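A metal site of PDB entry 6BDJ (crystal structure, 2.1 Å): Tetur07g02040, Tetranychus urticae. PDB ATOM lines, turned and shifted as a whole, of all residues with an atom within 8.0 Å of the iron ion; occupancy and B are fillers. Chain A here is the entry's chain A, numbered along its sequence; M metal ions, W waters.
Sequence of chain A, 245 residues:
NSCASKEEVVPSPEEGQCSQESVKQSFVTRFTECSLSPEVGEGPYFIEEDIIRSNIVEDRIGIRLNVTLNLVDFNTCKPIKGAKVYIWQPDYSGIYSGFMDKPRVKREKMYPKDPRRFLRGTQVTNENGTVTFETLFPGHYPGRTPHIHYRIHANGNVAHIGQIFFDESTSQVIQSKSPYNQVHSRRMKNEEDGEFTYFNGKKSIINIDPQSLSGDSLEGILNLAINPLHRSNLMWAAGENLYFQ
A ring nitrogen (ND1) of His 147 is in hydrogen-bond range of the backbone carbonyl oxygen (O) of Thr 145 (2.7 Å).
The backbone carbonyl oxygen (O) of Trp 88 is in hydrogen-bond range of the backbone NH (N) of His 149 (2.9 Å).
O of Glu 42 lies close to ND1 of His 149, 3.1 Å away.
The iron ion is bound by the side-chain hydroxyl (OH) of Tyr 96 (1.9 Å), water W1 (2.2 Å), a ring nitrogen (NE2) of His 149 (2.3 Å) and a ring nitrogen (NE2) of His 147 (2.5 Å).
The iron ion has four donor atoms within binding distance.
Three residues have an atom within 4 Å of the iron ion: Tyr 96, His 147 and His 149.
Along chain A the residues within 4 Å of the iron ion span positions 96 to 149.
The nearest printed residue that does not touch the iron ion is Arg 144 (4.5 Å).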
ATOM      1  N   GLY A  41      20.048 -20.536 -22.822  1.00  0.00           N
ATOM      2  CA  GLY A  41      19.319 -21.250 -23.871  1.00  0.00           C
ATOM      3  C   GLY A  41      17.971 -21.803 -23.370  1.00  0.00           C
ATOM      4  O   GLY A  41      17.830 -22.199 -22.226  1.00  0.00           O
ATOM      5  N   GLU A  42      16.990 -21.800 -24.259  1.00  0.00           N
ATOM      6  CA  GLU A  42      15.632 -22.244 -23.951  1.00  0.00           C
ATOM      7  C   GLU A  42      15.553 -23.724 -23.616  1.00  0.00           C
ATOM      8  O   GLU A  42      14.661 -24.156 -22.857  1.00  0.00           O
ATOM      9  CB  GLU A  42      14.779 -22.002 -25.178  1.00  0.00           C
ATOM     10  CG  GLU A  42      13.304 -22.223 -24.979  1.00  0.00           C
ATOM     11  CD  GLU A  42      12.543 -21.677 -26.171  1.00  0.00           C
ATOM     12  OE1 GLU A  42      12.397 -22.410 -27.199  1.00  0.00           O
ATOM     13  OE2 GLU A  42      12.100 -20.509 -26.074  1.00  0.00           O
ATOM     14  N   GLY A  43      16.454 -24.492 -24.216  1.00  0.00           N
ATOM     15  CA  GLY A  43      16.322 -25.936 -24.266  1.00  0.00           C
ATOM     16  C   GLY A  43      15.141 -26.331 -25.146  1.00  0.00           C
ATOM     17  O   GLY A  43      14.499 -25.474 -25.749  1.00  0.00           O
ATOM     18  N   PRO A  44      14.857 -27.637 -25.218  1.00  0.00           N
ATOM     19  CA  PRO A  44      13.896 -28.181 -26.168  1.00  0.00           C
ATOM     20  C   PRO A  44      12.435 -28.256 -25.752  1.00  0.00           C
ATOM     21  O   PRO A  44      11.612 -28.658 -26.563  1.00  0.00           O
ATOM     22  CB  PRO A  44      14.412 -29.619 -26.392  1.00  0.00           C
ATOM     23  CG  PRO A  44      15.414 -29.889 -25.306  1.00  0.00           C
ATOM     24  CD  PRO A  44      15.485 -28.696 -24.412  1.00  0.00           C
ATOM     25  N   TYR A  45      12.112 -27.886 -24.519  1.00  0.00           N
ATOM     26  CA  TYR A  45      10.776 -28.185 -23.997  1.00  0.00           C
ATOM     27  C   TYR A  45       9.838 -27.015 -23.774  1.00  0.00           C
ATOM     28  O   TYR A  45       8.811 -27.190 -23.087  1.00  0.00           O
ATOM     29  CB  TYR A  45      10.894 -29.031 -22.731  1.00  0.00           C
ATOM     30  CG  TYR A  45      11.740 -30.280 -22.931  1.00  0.00           C
ATOM     31  CD1 TYR A  45      11.502 -31.159 -24.000  1.00  0.00           C
ATOM     32  CD2 TYR A  45      12.786 -30.570 -22.072  1.00  0.00           C
ATOM     33  CE1 TYR A  45      12.258 -32.304 -24.171  1.00  0.00           C
ATOM     34  CE2 TYR A  45      13.575 -31.723 -22.238  1.00  0.00           C
ATOM     35  CZ  TYR A  45      13.302 -32.583 -23.282  1.00  0.00           C
ATOM     36  OH  TYR A  45      14.074 -33.712 -23.441  1.00  0.00           O
ATOM     37  N   PHE A  46      10.107 -25.878 -24.407  1.00  0.00           N
ATOM     38  CA  PHE A  46       9.130 -24.774 -24.358  1.00  0.00           C
ATOM     39  C   PHE A  46       7.912 -25.165 -25.140  1.00  0.00           C
ATOM     40  O   PHE A  46       8.011 -25.799 -26.208  1.00  0.00           O
ATOM     41  CB  PHE A  46       9.686 -23.451 -24.889  1.00  0.00           C
ATOM     42  CG  PHE A  46       8.722 -22.306 -24.759  1.00  0.00           C
ATOM     43  CD1 PHE A  46       8.195 -21.946 -23.510  1.00  0.00           C
ATOM     44  CD2 PHE A  46       8.303 -21.582 -25.872  1.00  0.00           C
ATOM     45  CE1 PHE A  46       7.294 -20.901 -23.393  1.00  0.00           C
ATOM     46  CE2 PHE A  46       7.421 -20.538 -25.760  1.00  0.00           C
ATOM     47  CZ  PHE A  46       6.899 -20.185 -24.531  1.00  0.00           C
ATOM     48  N   TRP A  88       8.569 -22.935 -17.046  1.00  0.00           N
ATOM     49  CA  TRP A  88       8.376 -24.357 -17.176  1.00  0.00           C
ATOM     50  C   TRP A  88       9.540 -25.074 -16.552  1.00  0.00           C
ATOM     51  O   TRP A  88      10.673 -24.565 -16.500  1.00  0.00           O
ATOM     52  CB  TRP A  88       8.131 -24.804 -18.630  1.00  0.00           C
ATOM     53  CG  TRP A  88       9.340 -24.669 -19.608  1.00  0.00           C
ATOM     54  CD1 TRP A  88      10.084 -25.681 -20.191  1.00  0.00           C
ATOM     55  CD2 TRP A  88       9.844 -23.449 -20.151  1.00  0.00           C
ATOM     56  NE1 TRP A  88      11.020 -25.154 -21.044  1.00  0.00           N
ATOM     57  CE2 TRP A  88      10.912 -23.793 -21.027  1.00  0.00           C
ATOM     58  CE3 TRP A  88       9.530 -22.103 -19.960  1.00  0.00           C
ATOM     59  CZ2 TRP A  88      11.648 -22.819 -21.729  1.00  0.00           C
ATOM     60  CZ3 TRP A  88      10.267 -21.148 -20.655  1.00  0.00           C
ATOM     61  CH2 TRP A  88      11.304 -21.512 -21.525  1.00  0.00           C
ATOM     62  N   GLN A  89       9.231 -26.252 -16.024  1.00  0.00           N
ATOM     63  CA  GLN A  89      10.200 -26.994 -15.225  1.00  0.00           C
ATOM     64  C   GLN A  89       9.814 -28.471 -15.203  1.00  0.00           C
ATOM     65  O   GLN A  89       8.660 -28.838 -15.414  1.00  0.00           O
ATOM     66  CB  GLN A  89      10.225 -26.429 -13.810  1.00  0.00           C
ATOM     67  CG  GLN A  89       8.958 -26.722 -13.022  1.00  0.00           C
ATOM     68  CD  GLN A  89       8.948 -26.133 -11.628  1.00  0.00           C
ATOM     69  OE1 GLN A  89       8.776 -24.938 -11.452  1.00  0.00           O
ATOM     70  NE2 GLN A  89       9.069 -26.995 -10.634  1.00  0.00           N
ATOM     71  N   PRO A  90      10.764 -29.334 -14.894  1.00  0.00           N
ATOM     72  CA  PRO A  90      10.399 -30.745 -14.727  1.00  0.00           C
ATOM     73  C   PRO A  90       9.855 -31.088 -13.357  1.00  0.00           C
ATOM     74  O   PRO A  90      10.173 -30.389 -12.375  1.00  0.00           O
ATOM     75  CB  PRO A  90      11.715 -31.460 -14.931  1.00  0.00           C
ATOM     76  CG  PRO A  90      12.746 -30.500 -14.470  1.00  0.00           C
ATOM     77  CD  PRO A  90      12.196 -29.112 -14.606  1.00  0.00           C
ATOM     78  N   GLY A  94      12.175 -35.544 -12.950  1.00  0.00           N
ATOM     79  CA  GLY A  94      12.764 -34.989 -14.159  1.00  0.00           C
ATOM     80  C   GLY A  94      11.969 -35.026 -15.450  1.00  0.00           C
ATOM     81  O   GLY A  94      12.572 -34.912 -16.526  1.00  0.00           O
ATOM     82  N   TYR A  96       9.157 -33.530 -18.092  1.00  0.00           N
ATOM     83  CA  TYR A  96       8.496 -32.340 -18.574  1.00  0.00           C
ATOM     84  C   TYR A  96       7.151 -32.728 -19.167  1.00  0.00           C
ATOM     85  O   TYR A  96       7.085 -33.649 -19.991  1.00  0.00           O
ATOM     86  CB  TYR A  96       9.309 -31.672 -19.668  1.00  0.00           C
ATOM     87  CG  TYR A  96      10.480 -30.875 -19.139  1.00  0.00           C
ATOM     88  CD1 TYR A  96      10.331 -29.577 -18.776  1.00  0.00           C
ATOM     89  CD2 TYR A  96      11.737 -31.472 -18.996  1.00  0.00           C
ATOM     90  CE1 TYR A  96      11.402 -28.825 -18.302  1.00  0.00           C
ATOM     91  CE2 TYR A  96      12.825 -30.734 -18.533  1.00  0.00           C
ATOM     92  CZ  TYR A  96      12.663 -29.401 -18.190  1.00  0.00           C
ATOM     93  OH  TYR A  96      13.714 -28.698 -17.703  1.00  0.00           O
ATOM     94  N   GLY A 139      12.645 -31.084 -10.022  1.00  0.00           N
ATOM     95  CA  GLY A 139      13.566 -32.218 -10.121  1.00  0.00           C
ATOM     96  C   GLY A 139      14.596 -31.849 -11.172  1.00  0.00           C
ATOM     97  O   GLY A 139      14.776 -30.680 -11.516  1.00  0.00           O
ATOM     98  N   HIS A 140      15.285 -32.839 -11.693  1.00  0.00           N
ATOM     99  CA  HIS A 140      16.198 -32.559 -12.776  1.00  0.00           C
ATOM    100  C   HIS A 140      16.452 -33.769 -13.567  1.00  0.00           C
ATOM    101  O   HIS A 140      16.333 -34.917 -13.115  1.00  0.00           O
ATOM    102  CB  HIS A 140      17.570 -32.095 -12.265  1.00  0.00           C
ATOM    103  CG  HIS A 140      18.158 -32.987 -11.212  1.00  0.00           C
ATOM    104  ND1 HIS A 140      19.003 -34.038 -11.510  1.00  0.00           N
ATOM    105  CD2 HIS A 140      18.002 -32.998  -9.869  1.00  0.00           C
ATOM    106  CE1 HIS A 140      19.337 -34.656 -10.393  1.00  0.00           C
ATOM    107  NE2 HIS A 140      18.757 -34.035  -9.383  1.00  0.00           N
ATOM    108  N   TYR A 141      17.033 -33.497 -14.731  1.00  0.00           N
ATOM    109  CA  TYR A 141      17.472 -34.490 -15.669  1.00  0.00           C
ATOM    110  C   TYR A 141      18.826 -35.023 -15.279  1.00  0.00           C
ATOM    111  O   TYR A 141      19.428 -34.562 -14.296  1.00  0.00           O
ATOM    112  CB  TYR A 141      17.628 -33.758 -17.001  1.00  0.00           C
ATOM    113  CG  TYR A 141      16.557 -34.067 -18.000  1.00  0.00           C
ATOM    114  CD1 TYR A 141      15.241 -33.833 -17.710  1.00  0.00           C
ATOM    115  CD2 TYR A 141      16.869 -34.598 -19.234  1.00  0.00           C
ATOM    116  CE1 TYR A 141      14.246 -34.097 -18.625  1.00  0.00           C
ATOM    117  CE2 TYR A 141      15.882 -34.885 -20.154  1.00  0.00           C
ATOM    118  CZ  TYR A 141      14.573 -34.631 -19.840  1.00  0.00           C
ATOM    119  OH  TYR A 141      13.545 -34.904 -20.721  1.00  0.00           O
ATOM    120  N   ARG A 144      22.166 -32.435 -16.223  1.00  0.00           N
ATOM    121  CA  ARG A 144      21.711 -31.080 -15.940  1.00  0.00           C
ATOM    122  C   ARG A 144      21.536 -30.874 -14.443  1.00  0.00           C
ATOM    123  O   ARG A 144      21.114 -31.762 -13.707  1.00  0.00           O
ATOM    124  CB  ARG A 144      20.360 -30.783 -16.617  1.00  0.00           C
ATOM    125  CG  ARG A 144      20.420 -30.625 -18.134  1.00  0.00           C
ATOM    126  CD  ARG A 144      21.330 -29.485 -18.605  1.00  0.00           C
ATOM    127  NE  ARG A 144      21.308 -28.288 -17.752  1.00  0.00           N
ATOM    128  CZ  ARG A 144      20.539 -27.214 -17.938  1.00  0.00           C
ATOM    129  NH1 ARG A 144      20.647 -26.199 -17.095  1.00  0.00           N
ATOM    130  NH2 ARG A 144      19.674 -27.160 -18.956  1.00  0.00           N
ATOM    131  N   THR A 145      21.831 -29.658 -14.018  1.00  0.00           N
ATOM    132  CA  THR A 145      21.626 -29.248 -12.656  1.00  0.00           C
ATOM    133  C   THR A 145      20.161 -28.769 -12.529  1.00  0.00           C
ATOM    134  O   THR A 145      19.537 -28.396 -13.538  1.00  0.00           O
ATOM    135  CB  THR A 145      22.653 -28.162 -12.287  1.00  0.00           C
ATOM    136  OG1 THR A 145      22.468 -27.721 -10.932  1.00  0.00           O
ATOM    137  CG2 THR A 145      22.627 -26.975 -13.278  1.00  0.00           C
ATOM    138  N   PRO A 146      19.604 -28.770 -11.299  1.00  0.00           N
ATOM    139  CA  PRO A 146      18.180 -28.402 -11.185  1.00  0.00           C
ATOM    140  C   PRO A 146      17.955 -26.949 -11.569  1.00  0.00           C
ATOM    141  O   PRO A 146      18.760 -26.096 -11.236  1.00  0.00           O
ATOM    142  CB  PRO A 146      17.861 -28.619  -9.695  1.00  0.00           C
ATOM    143  CG  PRO A 146      18.903 -29.551  -9.208  1.00  0.00           C
ATOM    144  CD  PRO A 146      20.131 -29.270 -10.025  1.00  0.00           C
ATOM    145  N   HIS A 147      16.864 -26.696 -12.268  1.00  0.00           N
ATOM    146  CA  HIS A 147      16.548 -25.348 -12.697  1.00  0.00           C
ATOM    147  C   HIS A 147      15.109 -25.221 -13.107  1.00  0.00           C
ATOM    148  O   HIS A 147      14.430 -26.218 -13.353  1.00  0.00           O
ATOM    149  CB  HIS A 147      17.367 -25.007 -13.921  1.00  0.00           C
ATOM    150  CG  HIS A 147      17.161 -25.960 -15.048  1.00  0.00           C
ATOM    151  ND1 HIS A 147      17.792 -27.170 -15.126  1.00  0.00           N
ATOM    152  CD2 HIS A 147      16.352 -25.888 -16.133  1.00  0.00           C
ATOM    153  CE1 HIS A 147      17.436 -27.790 -16.238  1.00  0.00           C
ATOM    154  NE2 HIS A 147      16.517 -27.057 -16.838  1.00  0.00           N
ATOM    155  N   ILE A 148      14.689 -23.963 -13.228  1.00  0.00           N
ATOM    156  CA  ILE A 148      13.399 -23.604 -13.802  1.00  0.00           C
ATOM    157  C   ILE A 148      13.662 -22.689 -14.969  1.00  0.00           C
ATOM    158  O   ILE A 148      14.405 -21.691 -14.840  1.00  0.00           O
ATOM    159  CB  ILE A 148      12.531 -22.859 -12.782  1.00  0.00           C
ATOM    160  CG1 ILE A 148      12.181 -23.767 -11.593  1.00  0.00           C
ATOM    161  CG2 ILE A 148      11.232 -22.348 -13.433  1.00  0.00           C
ATOM    162  CD1 ILE A 148      11.518 -23.079 -10.398  1.00  0.00           C
ATOM    163  N   HIS A 149      13.052 -22.986 -16.112  1.00  0.00           N
ATOM    164  CA  HIS A 149      13.137 -22.104 -17.238  1.00  0.00           C
ATOM    165  C   HIS A 149      12.157 -20.971 -17.167  1.00  0.00           C
ATOM    166  O   HIS A 149      11.092 -21.122 -16.556  1.00  0.00           O
ATOM    167  CB  HIS A 149      12.789 -22.812 -18.497  1.00  0.00           C
ATOM    168  CG  HIS A 149      13.709 -23.905 -18.855  1.00  0.00           C
ATOM    169  ND1 HIS A 149      14.739 -23.732 -19.775  1.00  0.00           N
ATOM    170  CD2 HIS A 149      13.734 -25.198 -18.488  1.00  0.00           C
ATOM    171  CE1 HIS A 149      15.362 -24.879 -19.941  1.00  0.00           C
ATOM    172  NE2 HIS A 149      14.773 -25.778 -19.165  1.00  0.00           N
ATOM    173  N   GLN A 163      17.180 -19.127 -17.311  1.00  0.00           N
ATOM    174  CA  GLN A 163      17.056 -20.239 -16.395  1.00  0.00           C
ATOM    175  C   GLN A 163      17.331 -19.749 -15.000  1.00  0.00           C
ATOM    176  O   GLN A 163      18.227 -18.949 -14.783  1.00  0.00           O
ATOM    177  CB  GLN A 163      18.020 -21.352 -16.781  1.00  0.00           C
ATOM    178  CG  GLN A 163      17.585 -22.068 -18.056  1.00  0.00           C
ATOM    179  CD  GLN A 163      18.443 -23.263 -18.424  1.00  0.00           C
ATOM    180  OE1 GLN A 163      19.085 -23.873 -17.562  1.00  0.00           O
ATOM    181  NE2 GLN A 163      18.454 -23.599 -19.715  1.00  0.00           N
ATOM    182  N   GLU A 195      25.439 -25.132 -19.401  1.00  0.00           N
ATOM    183  CA  GLU A 195      24.622 -23.940 -19.442  1.00  0.00           C
ATOM    184  C   GLU A 195      24.949 -22.964 -18.292  1.00  0.00           C
ATOM    185  O   GLU A 195      25.104 -21.779 -18.535  1.00  0.00           O
ATOM    186  CB  GLU A 195      23.116 -24.274 -19.456  1.00  0.00           C
ATOM    187  CG  GLU A 195      22.621 -25.248 -20.615  1.00  0.00           C
ATOM    188  CD  GLU A 195      21.975 -24.506 -21.893  1.00  0.00           C
ATOM    189  OE1 GLU A 195      20.975 -25.048 -22.467  1.00  0.00           O
ATOM    190  OE2 GLU A 195      22.442 -23.379 -22.312  1.00  0.00           O
HETATM  191 FE    FE M   1      15.232 -28.030 -18.706  1.00  0.00          FE
HETATM  192  O   HOH W   1      15.133 -28.297 -20.857  1.00  0.00           O
HETATM  193  O   HOH W   2      17.883 -27.959 -20.949  1.00  0.00           O
